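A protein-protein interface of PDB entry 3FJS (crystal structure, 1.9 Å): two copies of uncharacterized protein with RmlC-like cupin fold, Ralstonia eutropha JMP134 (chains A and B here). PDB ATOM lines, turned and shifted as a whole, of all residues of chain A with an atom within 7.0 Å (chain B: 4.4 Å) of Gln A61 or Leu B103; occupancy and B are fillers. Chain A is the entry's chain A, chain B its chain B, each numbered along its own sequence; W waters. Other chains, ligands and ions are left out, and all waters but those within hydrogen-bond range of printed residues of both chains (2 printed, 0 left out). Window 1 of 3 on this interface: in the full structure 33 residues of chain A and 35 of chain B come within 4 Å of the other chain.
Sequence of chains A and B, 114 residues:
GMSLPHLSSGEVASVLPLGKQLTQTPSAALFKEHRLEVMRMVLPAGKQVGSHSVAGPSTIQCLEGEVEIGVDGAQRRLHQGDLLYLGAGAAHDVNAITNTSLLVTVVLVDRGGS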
ATOM      1  N   VAL A  15       8.437  20.205  18.825  1.00  0.00           N
ATOM      2  CA  VAL A  15       7.135  20.056  18.147  1.00  0.00           C
ATOM      3  C   VAL A  15       6.202  19.153  18.930  1.00  0.00           C
ATOM      4  O   VAL A  15       5.300  18.545  18.355  1.00  0.00           O
ATOM      5  CB  VAL A  15       7.255  19.661  16.627  1.00  0.00           C
ATOM      6  CG1 VAL A  15       7.999  20.775  15.892  1.00  0.00           C
ATOM      7  CG2 VAL A  15       7.924  18.287  16.414  1.00  0.00           C
ATOM      8  N   THR A  59       5.398  17.542   3.190  1.00  0.00           N
ATOM      9  CA  THR A  59       4.827  16.617   4.138  1.00  0.00           C
ATOM     10  C   THR A  59       4.052  17.382   5.177  1.00  0.00           C
ATOM     11  O   THR A  59       4.434  18.511   5.558  1.00  0.00           O
ATOM     12  CB  THR A  59       5.851  15.646   4.838  1.00  0.00           C
ATOM     13  OG1 THR A  59       6.803  16.377   5.650  1.00  0.00           O
ATOM     14  CG2 THR A  59       6.580  14.786   3.823  1.00  0.00           C
ATOM     15  N   ILE A  60       2.968  16.772   5.623  1.00  0.00           N
ATOM     16  CA  ILE A  60       2.122  17.331   6.665  1.00  0.00           C
ATOM     17  C   ILE A  60       1.986  16.254   7.747  1.00  0.00           C
ATOM     18  O   ILE A  60       1.472  15.160   7.483  1.00  0.00           O
ATOM     19  CB  ILE A  60       0.721  17.752   6.142  1.00  0.00           C
ATOM     20  CG1 ILE A  60       0.791  18.815   5.025  1.00  0.00           C
ATOM     21  CG2 ILE A  60      -0.149  18.260   7.292  1.00  0.00           C
ATOM     22  CD1 ILE A  60      -0.643  19.205   4.435  1.00  0.00           C
ATOM     23  N   GLN A  61       2.464  16.566   8.954  1.00  0.00           N
ATOM     24  CA  GLN A  61       2.390  15.674  10.088  1.00  0.00           C
ATOM     25  C   GLN A  61       1.428  16.256  11.083  1.00  0.00           C
ATOM     26  O   GLN A  61       1.559  17.426  11.470  1.00  0.00           O
ATOM     27  CB  GLN A  61       3.758  15.526  10.733  1.00  0.00           C
ATOM     28  CG  GLN A  61       3.827  14.558  11.903  1.00  0.00           C
ATOM     29  CD  GLN A  61       5.194  14.507  12.537  1.00  0.00           C
ATOM     30  OE1 GLN A  61       6.219  14.789  11.899  1.00  0.00           O
ATOM     31  NE2 GLN A  61       5.220  14.151  13.821  1.00  0.00           N
ATOM     32  N   CYS A  62       0.483  15.442  11.518  1.00  0.00           N
ATOM     33  CA  CYS A  62      -0.501  15.857  12.529  1.00  0.00           C
ATOM     34  C   CYS A  62       0.109  15.616  13.927  1.00  0.00           C
ATOM     35  O   CYS A  62       0.306  14.484  14.342  1.00  0.00           O
ATOM     36  CB  CYS A  62      -1.777  15.090  12.367  1.00  0.00           C
ATOM     37  SG  CYS A  62      -3.044  15.486  13.582  1.00  0.00           S
ATOM     38  N   LEU A  63       0.398  16.697  14.635  1.00  0.00           N
ATOM     39  CA  LEU A  63       1.109  16.640  15.948  1.00  0.00           C
ATOM     40  C   LEU A  63       0.144  16.363  17.098  1.00  0.00           C
ATOM     41  O   LEU A  63       0.521  15.755  18.128  1.00  0.00           O
ATOM     42  CB  LEU A  63       1.895  17.924  16.185  1.00  0.00           C
ATOM     43  CG  LEU A  63       2.938  18.325  15.111  1.00  0.00           C
ATOM     44  CD1 LEU A  63       3.443  19.737  15.342  1.00  0.00           C
ATOM     45  CD2 LEU A  63       4.098  17.337  15.047  1.00  0.00           C
ATOM     46  N   GLU A  64      -1.102  16.769  16.926  1.00  0.00           N
ATOM     47  CA  GLU A  64      -2.148  16.567  17.940  1.00  0.00           C
ATOM     48  C   GLU A  64      -3.495  16.883  17.301  1.00  0.00           C
ATOM     49  O   GLU A  64      -3.570  17.593  16.275  1.00  0.00           O
ATOM     50  CB  GLU A  64      -1.911  17.488  19.135  1.00  0.00           C
ATOM     51  CG  GLU A  64      -2.076  18.962  18.817  1.00  0.00           C
ATOM     52  CD  GLU A  64      -1.518  19.857  19.880  1.00  0.00           C
ATOM     53  OE1 GLU A  64      -1.924  19.757  21.055  1.00  0.00           O
ATOM     54  OE2 GLU A  64      -0.690  20.697  19.510  1.00  0.00           O
ATOM     55  N   VAL A  67      -7.397  16.469  11.807  1.00  0.00           N
ATOM     56  CA  VAL A  67      -7.498  17.345  10.652  1.00  0.00           C
ATOM     57  C   VAL A  67      -7.876  16.512   9.445  1.00  0.00           C
ATOM     58  O   VAL A  67      -7.477  15.359   9.341  1.00  0.00           O
ATOM     59  CB  VAL A  67      -6.138  18.055  10.429  1.00  0.00           C
ATOM     60  CG1 VAL A  67      -4.998  17.056  10.131  1.00  0.00           C
ATOM     61  CG2 VAL A  67      -6.221  19.118   9.334  1.00  0.00           C
ATOM     62  N   ILE A  69      -7.577  16.410   5.449  1.00  0.00           N
ATOM     63  CA  ILE A  69      -6.827  16.983   4.335  1.00  0.00           C
ATOM     64  C   ILE A  69      -7.403  16.371   3.074  1.00  0.00           C
ATOM     65  O   ILE A  69      -7.349  15.148   2.891  1.00  0.00           O
ATOM     66  CB  ILE A  69      -5.310  16.741   4.435  1.00  0.00           C
ATOM     67  CG1 ILE A  69      -4.733  17.429   5.689  1.00  0.00           C
ATOM     68  CG2 ILE A  69      -4.589  17.289   3.151  1.00  0.00           C
ATOM     69  CD1 ILE A  69      -3.491  16.852   6.125  1.00  0.00           C
ATOM     70  N   LEU A  78      -6.507  12.713   9.284  1.00  0.00           N
ATOM     71  CA  LEU A  78      -5.267  12.460  10.009  1.00  0.00           C
ATOM     72  C   LEU A  78      -5.487  12.580  11.506  1.00  0.00           C
ATOM     73  O   LEU A  78      -6.169  13.485  11.960  1.00  0.00           O
ATOM     74  CB  LEU A  78      -4.162  13.423   9.626  1.00  0.00           C
ATOM     75  CG  LEU A  78      -3.794  13.702   8.171  1.00  0.00           C
ATOM     76  CD1 LEU A  78      -2.435  14.384   8.127  1.00  0.00           C
ATOM     77  CD2 LEU A  78      -3.753  12.474   7.411  1.00  0.00           C
ATOM     78  N   HIS A  79      -4.878  11.676  12.253  1.00  0.00           N
ATOM     79  CA  HIS A  79      -4.868  11.700  13.711  1.00  0.00           C
ATOM     80  C   HIS A  79      -3.432  11.955  14.137  1.00  0.00           C
ATOM     81  O   HIS A  79      -2.551  11.994  13.297  1.00  0.00           O
ATOM     82  CB  HIS A  79      -5.363  10.383  14.259  1.00  0.00           C
ATOM     83  CG  HIS A  79      -6.819  10.148  13.988  1.00  0.00           C
ATOM     84  ND1 HIS A  79      -7.305   9.836  12.736  1.00  0.00           N
ATOM     85  CD2 HIS A  79      -7.901  10.223  14.796  1.00  0.00           C
ATOM     86  CE1 HIS A  79      -8.618   9.693  12.793  1.00  0.00           C
ATOM     87  NE2 HIS A  79      -9.004   9.923  14.032  1.00  0.00           N
ATOM     88  N   GLN A  80      -3.186  12.119  15.448  1.00  0.00           N
ATOM     89  CA  GLN A  80      -1.834  12.380  15.941  1.00  0.00           C
ATOM     90  C   GLN A  80      -0.882  11.314  15.438  1.00  0.00           C
ATOM     91  O   GLN A  80      -1.219  10.127  15.436  1.00  0.00           O
ATOM     92  CB  GLN A  80      -1.836  12.381  17.466  1.00  0.00           C
ATOM     93  CG  GLN A  80      -0.553  12.642  18.133  1.00  0.00           C
ATOM     94  CD  GLN A  80      -0.791  12.862  19.632  1.00  0.00           C
ATOM     95  OE1 GLN A  80      -1.416  12.031  20.272  1.00  0.00           O
ATOM     96  NE2 GLN A  80      -0.328  13.963  20.163  1.00  0.00           N
ATOM     97  N   GLY A  81       0.280  11.747  14.967  1.00  0.00           N
ATOM     98  CA  GLY A  81       1.284  10.827  14.431  1.00  0.00           C
ATOM     99  C   GLY A  81       1.149  10.511  12.948  1.00  0.00           C
ATOM    100  O   GLY A  81       2.052   9.926  12.402  1.00  0.00           O
ATOM    101  N   ASP A  82       0.068  10.941  12.297  1.00  0.00           N
ATOM    102  CA  ASP A  82      -0.106  10.659  10.873  1.00  0.00           C
ATOM    103  C   ASP A  82       0.723  11.622  10.061  1.00  0.00           C
ATOM    104  O   ASP A  82       0.727  12.823  10.335  1.00  0.00           O
ATOM    105  CB  ASP A  82      -1.528  10.710  10.439  1.00  0.00           C
ATOM    106  CG  ASP A  82      -2.320   9.506  10.908  1.00  0.00           C
ATOM    107  OD1 ASP A  82      -1.745   8.431  11.220  1.00  0.00           O
ATOM    108  OD2 ASP A  82      -3.540   9.648  10.968  1.00  0.00           O
ATOM    109  N   LEU A  83       1.397  11.057   9.071  1.00  0.00           N
ATOM    110  CA  LEU A  83       2.277  11.825   8.184  1.00  0.00           C
ATOM    111  C   LEU A  83       1.773  11.640   6.764  1.00  0.00           C
ATOM    112  O   LEU A  83       1.744  10.518   6.257  1.00  0.00           O
ATOM    113  CB  LEU A  83       3.736  11.388   8.313  1.00  0.00           C
ATOM    114  CG  LEU A  83       4.805  12.174   7.516  1.00  0.00           C
ATOM    115  CD1 LEU A  83       4.866  13.645   7.864  1.00  0.00           C
ATOM    116  CD2 LEU A  83       6.216  11.577   7.677  1.00  0.00           C
ATOM    117  N   LEU A  84       1.384  12.756   6.136  1.00  0.00           N
ATOM    118  CA  LEU A  84       0.871  12.782   4.757  1.00  0.00           C
ATOM    119  C   LEU A  84       1.960  13.286   3.827  1.00  0.00           C
ATOM    120  O   LEU A  84       2.561  14.332   4.088  1.00  0.00           O
ATOM    121  CB  LEU A  84      -0.354  13.712   4.630  1.00  0.00           C
ATOM    122  CG  LEU A  84      -0.879  14.069   3.241  1.00  0.00           C
ATOM    123  CD1 LEU A  84      -1.468  12.816   2.635  1.00  0.00           C
ATOM    124  CD2 LEU A  84      -1.890  15.206   3.362  1.00  0.00           C
ATOM    125  N   THR A 100      -5.848  21.670  16.474  1.00  0.00           N
ATOM    126  CA  THR A 100      -4.778  20.820  15.973  1.00  0.00           C
ATOM    127  C   THR A 100      -3.567  21.637  15.616  1.00  0.00           C
ATOM    128  O   THR A 100      -3.658  22.849  15.413  1.00  0.00           O
ATOM    129  CB  THR A 100      -5.336  20.013  14.724  1.00  0.00           C
ATOM    130  OG1 THR A 100      -4.395  19.060  14.249  1.00  0.00           O
ATOM    131  CG2 THR A 100      -5.764  20.945  13.589  1.00  0.00           C
ATOM    132  N   SER A 101      -2.397  20.987  15.645  1.00  0.00           N
ATOM    133  CA  SER A 101      -1.182  21.620  15.155  1.00  0.00           C
ATOM    134  C   SER A 101      -0.530  20.629  14.202  1.00  0.00           C
ATOM    135  O   SER A 101      -0.576  19.424  14.430  1.00  0.00           O
ATOM    136  CB  SER A 101      -0.283  22.107  16.292  1.00  0.00           C
ATOM    137  OG  SER A 101       0.225  21.047  17.057  1.00  0.00           O
ATOM    138  N   LEU A 102       0.071  21.174  13.143  1.00  0.00           N
ATOM    139  CA  LEU A 102       0.620  20.425  12.058  1.00  0.00           C
ATOM    140  C   LEU A 102       2.043  20.853  11.822  1.00  0.00           C
ATOM    141  O   LEU A 102       2.326  22.059  11.908  1.00  0.00           O
ATOM    142  CB  LEU A 102      -0.152  20.749  10.763  1.00  0.00           C
ATOM    143  CG  LEU A 102      -1.666  20.688  10.771  1.00  0.00           C
ATOM    144  CD1 LEU A 102      -2.230  21.087   9.337  1.00  0.00           C
ATOM    145  CD2 LEU A 102      -2.107  19.303  11.257  1.00  0.00           C
ATOM    146  N   LEU A 103       2.918  19.893  11.538  1.00  0.00           N
ATOM    147  CA  LEU A 103       4.307  20.199  11.182  1.00  0.00           C
ATOM    148  C   LEU A 103       4.276  20.081   9.672  1.00  0.00           C
ATOM    149  O   LEU A 103       4.002  18.991   9.159  1.00  0.00           O
ATOM    150  CB  LEU A 103       5.312  19.219  11.770  1.00  0.00           C
ATOM    151  CG  LEU A 103       6.785  19.548  11.507  1.00  0.00           C
ATOM    152  CD1 LEU A 103       7.122  20.897  12.147  1.00  0.00           C
ATOM    153  CD2 LEU A 103       7.649  18.417  12.081  1.00  0.00           C
ATOM    154  N   VAL A 104       4.566  21.178   8.993  1.00  0.00           N
ATOM    155  CA  VAL A 104       4.533  21.250   7.538  1.00  0.00           C
ATOM    156  C   VAL A 104       5.956  21.515   7.019  1.00  0.00           C
ATOM    157  O   VAL A 104       6.564  22.508   7.388  1.00  0.00           O
ATOM    158  CB  VAL A 104       3.506  22.333   7.054  1.00  0.00           C
ATOM    159  CG1 VAL A 104       3.421  22.362   5.527  1.00  0.00           C
ATOM    160  CG2 VAL A 104       2.110  22.106   7.658  1.00  0.00           C
ATOM    161  N   THR A 105       6.491  20.600   6.212  1.00  0.00           N
ATOM    162  CA  THR A 105       7.836  20.690   5.650  1.00  0.00           C
ATOM    163  C   THR A 105       7.657  20.805   4.133  1.00  0.00           C
ATOM    164  O   THR A 105       7.039  19.923   3.519  1.00  0.00           O
ATOM    165  CB  THR A 105       8.660  19.411   6.009  1.00  0.00           C
ATOM    166  OG1 THR A 105       8.679  19.210   7.437  1.00  0.00           O
ATOM    167  CG2 THR A 105      10.086  19.485   5.472  1.00  0.00           C
ATOM    168  N   VAL B  15       3.712   7.724  12.213  1.00  0.00           N
ATOM    169  CA  VAL B  15       5.024   7.842  12.906  1.00  0.00           C
ATOM    170  C   VAL B  15       4.807   7.976  14.433  1.00  0.00           C
ATOM    171  O   VAL B  15       5.629   8.559  15.161  1.00  0.00           O
ATOM    172  CB  VAL B  15       5.945   8.977  12.292  1.00  0.00           C
ATOM    173  CG1 VAL B  15       6.201   8.660  10.829  1.00  0.00           C
ATOM    174  CG2 VAL B  15       5.369  10.393  12.413  1.00  0.00           C
ATOM    175  N   LEU B  30       9.626   5.870   4.390  1.00  0.00           N
ATOM    176  CA  LEU B  30       8.187   6.190   4.189  1.00  0.00           C
ATOM    177  C   LEU B  30       8.010   6.384   2.703  1.00  0.00           C
ATOM    178  O   LEU B  30       7.070   5.875   2.104  1.00  0.00           O
ATOM    179  CB  LEU B  30       7.706   7.460   4.908  1.00  0.00           C
ATOM    180  CG  LEU B  30       7.257   7.378   6.372  1.00  0.00           C
ATOM    181  CD1 LEU B  30       8.405   7.082   7.320  1.00  0.00           C
ATOM    182  CD2 LEU B  30       6.564   8.690   6.767  1.00  0.00           C
ATOM    183  N   VAL B  38      11.957  10.442   3.008  1.00  0.00           N
ATOM    184  CA  VAL B  38      11.490  10.470   4.390  1.00  0.00           C
ATOM    185  C   VAL B  38      11.591   9.040   4.915  1.00  0.00           C
ATOM    186  O   VAL B  38      10.988   8.116   4.334  1.00  0.00           O
ATOM    187  CB  VAL B  38      10.105  11.080   4.516  1.00  0.00           C
ATOM    188  CG1 VAL B  38       9.610  11.015   5.958  1.00  0.00           C
ATOM    189  CG2 VAL B  38      10.128  12.532   4.088  1.00  0.00           C
ATOM    190  N   MET B  39      12.324   8.876   6.033  1.00  0.00           N
ATOM    191  CA  MET B  39      12.541   7.558   6.620  1.00  0.00           C
ATOM    192  C   MET B  39      12.403   7.559   8.133  1.00  0.00           C
ATOM    193  O   MET B  39      12.615   8.576   8.804  1.00  0.00           O
ATOM    194  CB  MET B  39      13.931   7.015   6.213  1.00  0.00           C
ATOM    195  CG  MET B  39      15.084   7.633   6.944  1.00  0.00           C
ATOM    196  SD  MET B  39      16.705   7.801   5.888  1.00  0.00           S
ATOM    197  CE  MET B  39      16.037   9.245   4.862  1.00  0.00           C
ATOM    198  N   THR B  59      16.064  17.350   8.247  1.00  0.00           N
ATOM    199  CA  THR B  59      15.529  17.456   9.606  1.00  0.00           C
ATOM    200  C   THR B  59      15.505  16.070  10.233  1.00  0.00           C
ATOM    201  O   THR B  59      15.274  15.045   9.539  1.00  0.00           O
ATOM    202  CB  THR B  59      14.143  18.145   9.709  1.00  0.00           C
ATOM    203  OG1 THR B  59      13.130  17.334   9.110  1.00  0.00           O
ATOM    204  CG2 THR B  59      14.160  19.574   9.059  1.00  0.00           C
ATOM    205  N   ILE B  60      15.835  16.039  11.513  1.00  0.00           N
ATOM    206  CA  ILE B  60      15.724  14.845  12.343  1.00  0.00           C
ATOM    207  C   ILE B  60      14.787  15.139  13.505  1.00  0.00           C
ATOM    208  O   ILE B  60      15.067  16.044  14.328  1.00  0.00           O
ATOM    209  CB  ILE B  60      17.079  14.415  12.943  1.00  0.00           C
ATOM    210  CG1 ILE B  60      18.093  14.157  11.822  1.00  0.00           C
ATOM    211  CG2 ILE B  60      16.884  13.173  13.837  1.00  0.00           C
ATOM    212  CD1 ILE B  60      19.535  13.923  12.333  1.00  0.00           C
ATOM    213  N   GLN B  61      13.701  14.363  13.589  1.00  0.00           N
ATOM    214  CA  GLN B  61      12.702  14.468  14.638  1.00  0.00           C
ATOM    215  C   GLN B  61      12.783  13.244  15.529  1.00  0.00           C
ATOM    216  O   GLN B  61      12.638  12.112  15.052  1.00  0.00           O
ATOM    217  CB  GLN B  61      11.292  14.616  14.069  1.00  0.00           C
ATOM    218  CG  GLN B  61      10.204  14.935  15.103  1.00  0.00           C
ATOM    219  CD  GLN B  61       8.815  14.981  14.490  1.00  0.00           C
ATOM    220  OE1 GLN B  61       7.836  14.585  15.127  1.00  0.00           O
ATOM    221  NE2 GLN B  61       8.729  15.419  13.224  1.00  0.00           N
ATOM    222  N   LEU B  63      11.142  10.872  17.730  1.00  0.00           N
ATOM    223  CA  LEU B  63       9.731  10.459  17.953  1.00  0.00           C
ATOM    224  C   LEU B  63       9.513   9.888  19.349  1.00  0.00           C
ATOM    225  O   LEU B  63       8.386   9.931  19.899  1.00  0.00           O
ATOM    226  CB  LEU B  63       9.289   9.445  16.900  1.00  0.00           C
ATOM    227  CG  LEU B  63       9.391   9.888  15.436  1.00  0.00           C
ATOM    228  CD1 LEU B  63       9.204   8.701  14.508  1.00  0.00           C
ATOM    229  CD2 LEU B  63       8.478  11.067  15.097  1.00  0.00           C
ATOM    230  N   LEU B 102      13.480   7.821  14.951  1.00  0.00           N
ATOM    231  CA  LEU B 102      13.663   9.165  14.428  1.00  0.00           C
ATOM    232  C   LEU B 102      12.967   9.302  13.102  1.00  0.00           C
ATOM    233  O   LEU B 102      13.032   8.354  12.301  1.00  0.00           O
ATOM    234  CB  LEU B 102      15.157   9.443  14.206  1.00  0.00           C
ATOM    235  CG  LEU B 102      16.146   9.093  15.313  1.00  0.00           C
ATOM    236  CD1 LEU B 102      17.561   9.384  14.835  1.00  0.00           C
ATOM    237  CD2 LEU B 102      15.807   9.862  16.579  1.00  0.00           C
ATOM    238  N   LEU B 103      12.308  10.435  12.846  1.00  0.00           N
ATOM    239  CA  LEU B 103      11.775  10.721  11.515  1.00  0.00           C
ATOM    240  C   LEU B 103      12.827  11.629  10.874  1.00  0.00           C
ATOM    241  O   LEU B 103      13.088  12.745  11.350  1.00  0.00           O
ATOM    242  CB  LEU B 103      10.436  11.436  11.552  1.00  0.00           C
ATOM    243  CG  LEU B 103       9.766  11.696  10.209  1.00  0.00           C
ATOM    244  CD1 LEU B 103       9.408  10.416   9.506  1.00  0.00           C
ATOM    245  CD2 LEU B 103       8.571  12.609  10.420  1.00  0.00           C
ATOM    246  N   VAL B 104      13.417  11.150   9.800  1.00  0.00           N
ATOM    247  CA  VAL B 104      14.490  11.848   9.105  1.00  0.00           C
ATOM    248  C   VAL B 104      13.998  12.240   7.732  1.00  0.00           C
ATOM    249  O   VAL B 104      13.627  11.362   6.971  1.00  0.00           O
ATOM    250  CB  VAL B 104      15.721  10.936   8.982  1.00  0.00           C
ATOM    251  CG1 VAL B 104      16.866  11.676   8.322  1.00  0.00           C
ATOM    252  CG2 VAL B 104      16.097  10.424  10.337  1.00  0.00           C
ATOM    253  N   THR B 105      13.990  13.548   7.451  1.00  0.00           N
ATOM    254  CA  THR B 105      13.512  14.109   6.182  1.00  0.00           C
ATOM    255  C   THR B 105      14.717  14.715   5.504  1.00  0.00           C
ATOM    256  O   THR B 105      15.328  15.615   6.085  1.00  0.00           O
ATOM    257  CB  THR B 105      12.438  15.156   6.459  1.00  0.00           C
ATOM    258  OG1 THR B 105      11.370  14.569   7.220  1.00  0.00           O
ATOM    259  CG2 THR B 105      11.885  15.708   5.164  1.00  0.00           C
HETATM  260  O   HOH W   1      10.650  18.398   9.279  1.00  0.00           O
HETATM  261  O   HOH W   2       8.497  14.743   6.893  1.00  0.00           O
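The side-chain amide oxygen (OE1) of Gln A61 is in hydrogen-bond range of the side-chain amide nitrogen (NE2) of Gln B61.
The backbone carbonyl oxygen (O) of Gly A81 sits at hydrogen-bond distance from the backbone NH (N) of Val B15 (2.8 Å).
Gln B61 touches Val A15 (OE1 to CG2, 3.9 Å).
Gln A61 touches Leu B103 (OE1 to CD2, 3.5 Å).
CD2 of Leu B30 touches CD2 of Leu A83 (3.0 Å).
CG1 of Val B38 touches CD2 of Leu A83 (3.8 Å).
Leu B103 touches Leu A83.
CD2 of Leu A103 touches NE2 of Gln B61, at 3.4 Å.
The backbone NH (N) of Leu A103 lies within hydrogen-bond range of the backbone carbonyl oxygen (O) of Gln A61, 2.8 Å away.
The backbone NH of Leu B103 sits at hydrogen-bond distance from the backbone carbonyl oxygen of Gln B61, 2.8 Å away.
The backbone NH (N) of Leu B30 lies within hydrogen-bond range of the backbone carbonyl oxygen (O) of Val B38 (2.6 Å).
The backbone carbonyl oxygen of Cys A62 sits at hydrogen-bond distance from the backbone NH of Gly A81, 2.8 Å away.
Printed residues of chain B within 4 Å of Val A15: Gln B61.
Of the printed residues of chain B, Gln A61 touches Gln B61 (2.9 Å) and Leu B103 (3.5 Å).
Cys A62 touches none of the printed residues of chain B.
Leu A78 touches none of the printed residues of chain B.
Printed residues of chain B within 4 Å of Gly A81: Val B15 (2.8 Å).
Of the printed residues of chain A, Val B15 touches Gly A81.
Of the printed residues of chain A, Leu B30 touches Leu A83.
Of the printed residues of chain A, Val B38 touches Leu A83 (3.8 Å).
Printed residues of chain A within 4 Å of Leu B103: Gln A61 (3.5 Å) and Leu A83 (3.8 Å).
The nearest printed residue of chain A that does not touch Leu B103 is Leu A103 (6.1 Å).
The nearest printed residue of chain B that does not touch Leu A103 is Leu B103 (6.1 Å).
Hydrophobic or aromatic side chains of chain A within 4 Å of the printed part of chain B: Val A15, Leu A83 and Leu A103.
Printed residues of chain B that touch a printed residue of chain A: Val B15, Leu B30, Val B38, Gln B61 and Leu B103.
Hydrophobic or aromatic side chains of chain B that line the printed part of chain A: Val B15, Leu B30, Val B38 and Leu B103.
Among the printed residues, 8 pairs touch across the chains.
Val A15 touches Gln B61, but with the chains exchanged Gln A61 does not touch Val B15 (4.02 Å).
Gln A61 touches its own counterpart, Gln B61.
Gln A61 touches Leu B103, and with the chains exchanged Leu A103 touches Gln B61.
Positions printed for both chains: 15, 59, 60, 61, 63, 102, 103, 104 and 105.
Of the 8 pairs that touch across the chains among the printed residues, 3 have their exchanged pair printed and touching as well.
Water W2 bridges the side-chain hydroxyl of Thr A59 (2.7 Å) and the side-chain hydroxyl of Thr B105 (2.9 Å).
Water W1 bridges OG1 of Thr B59 (2.7 Å) and OG1 of Thr A105 (2.8 Å).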
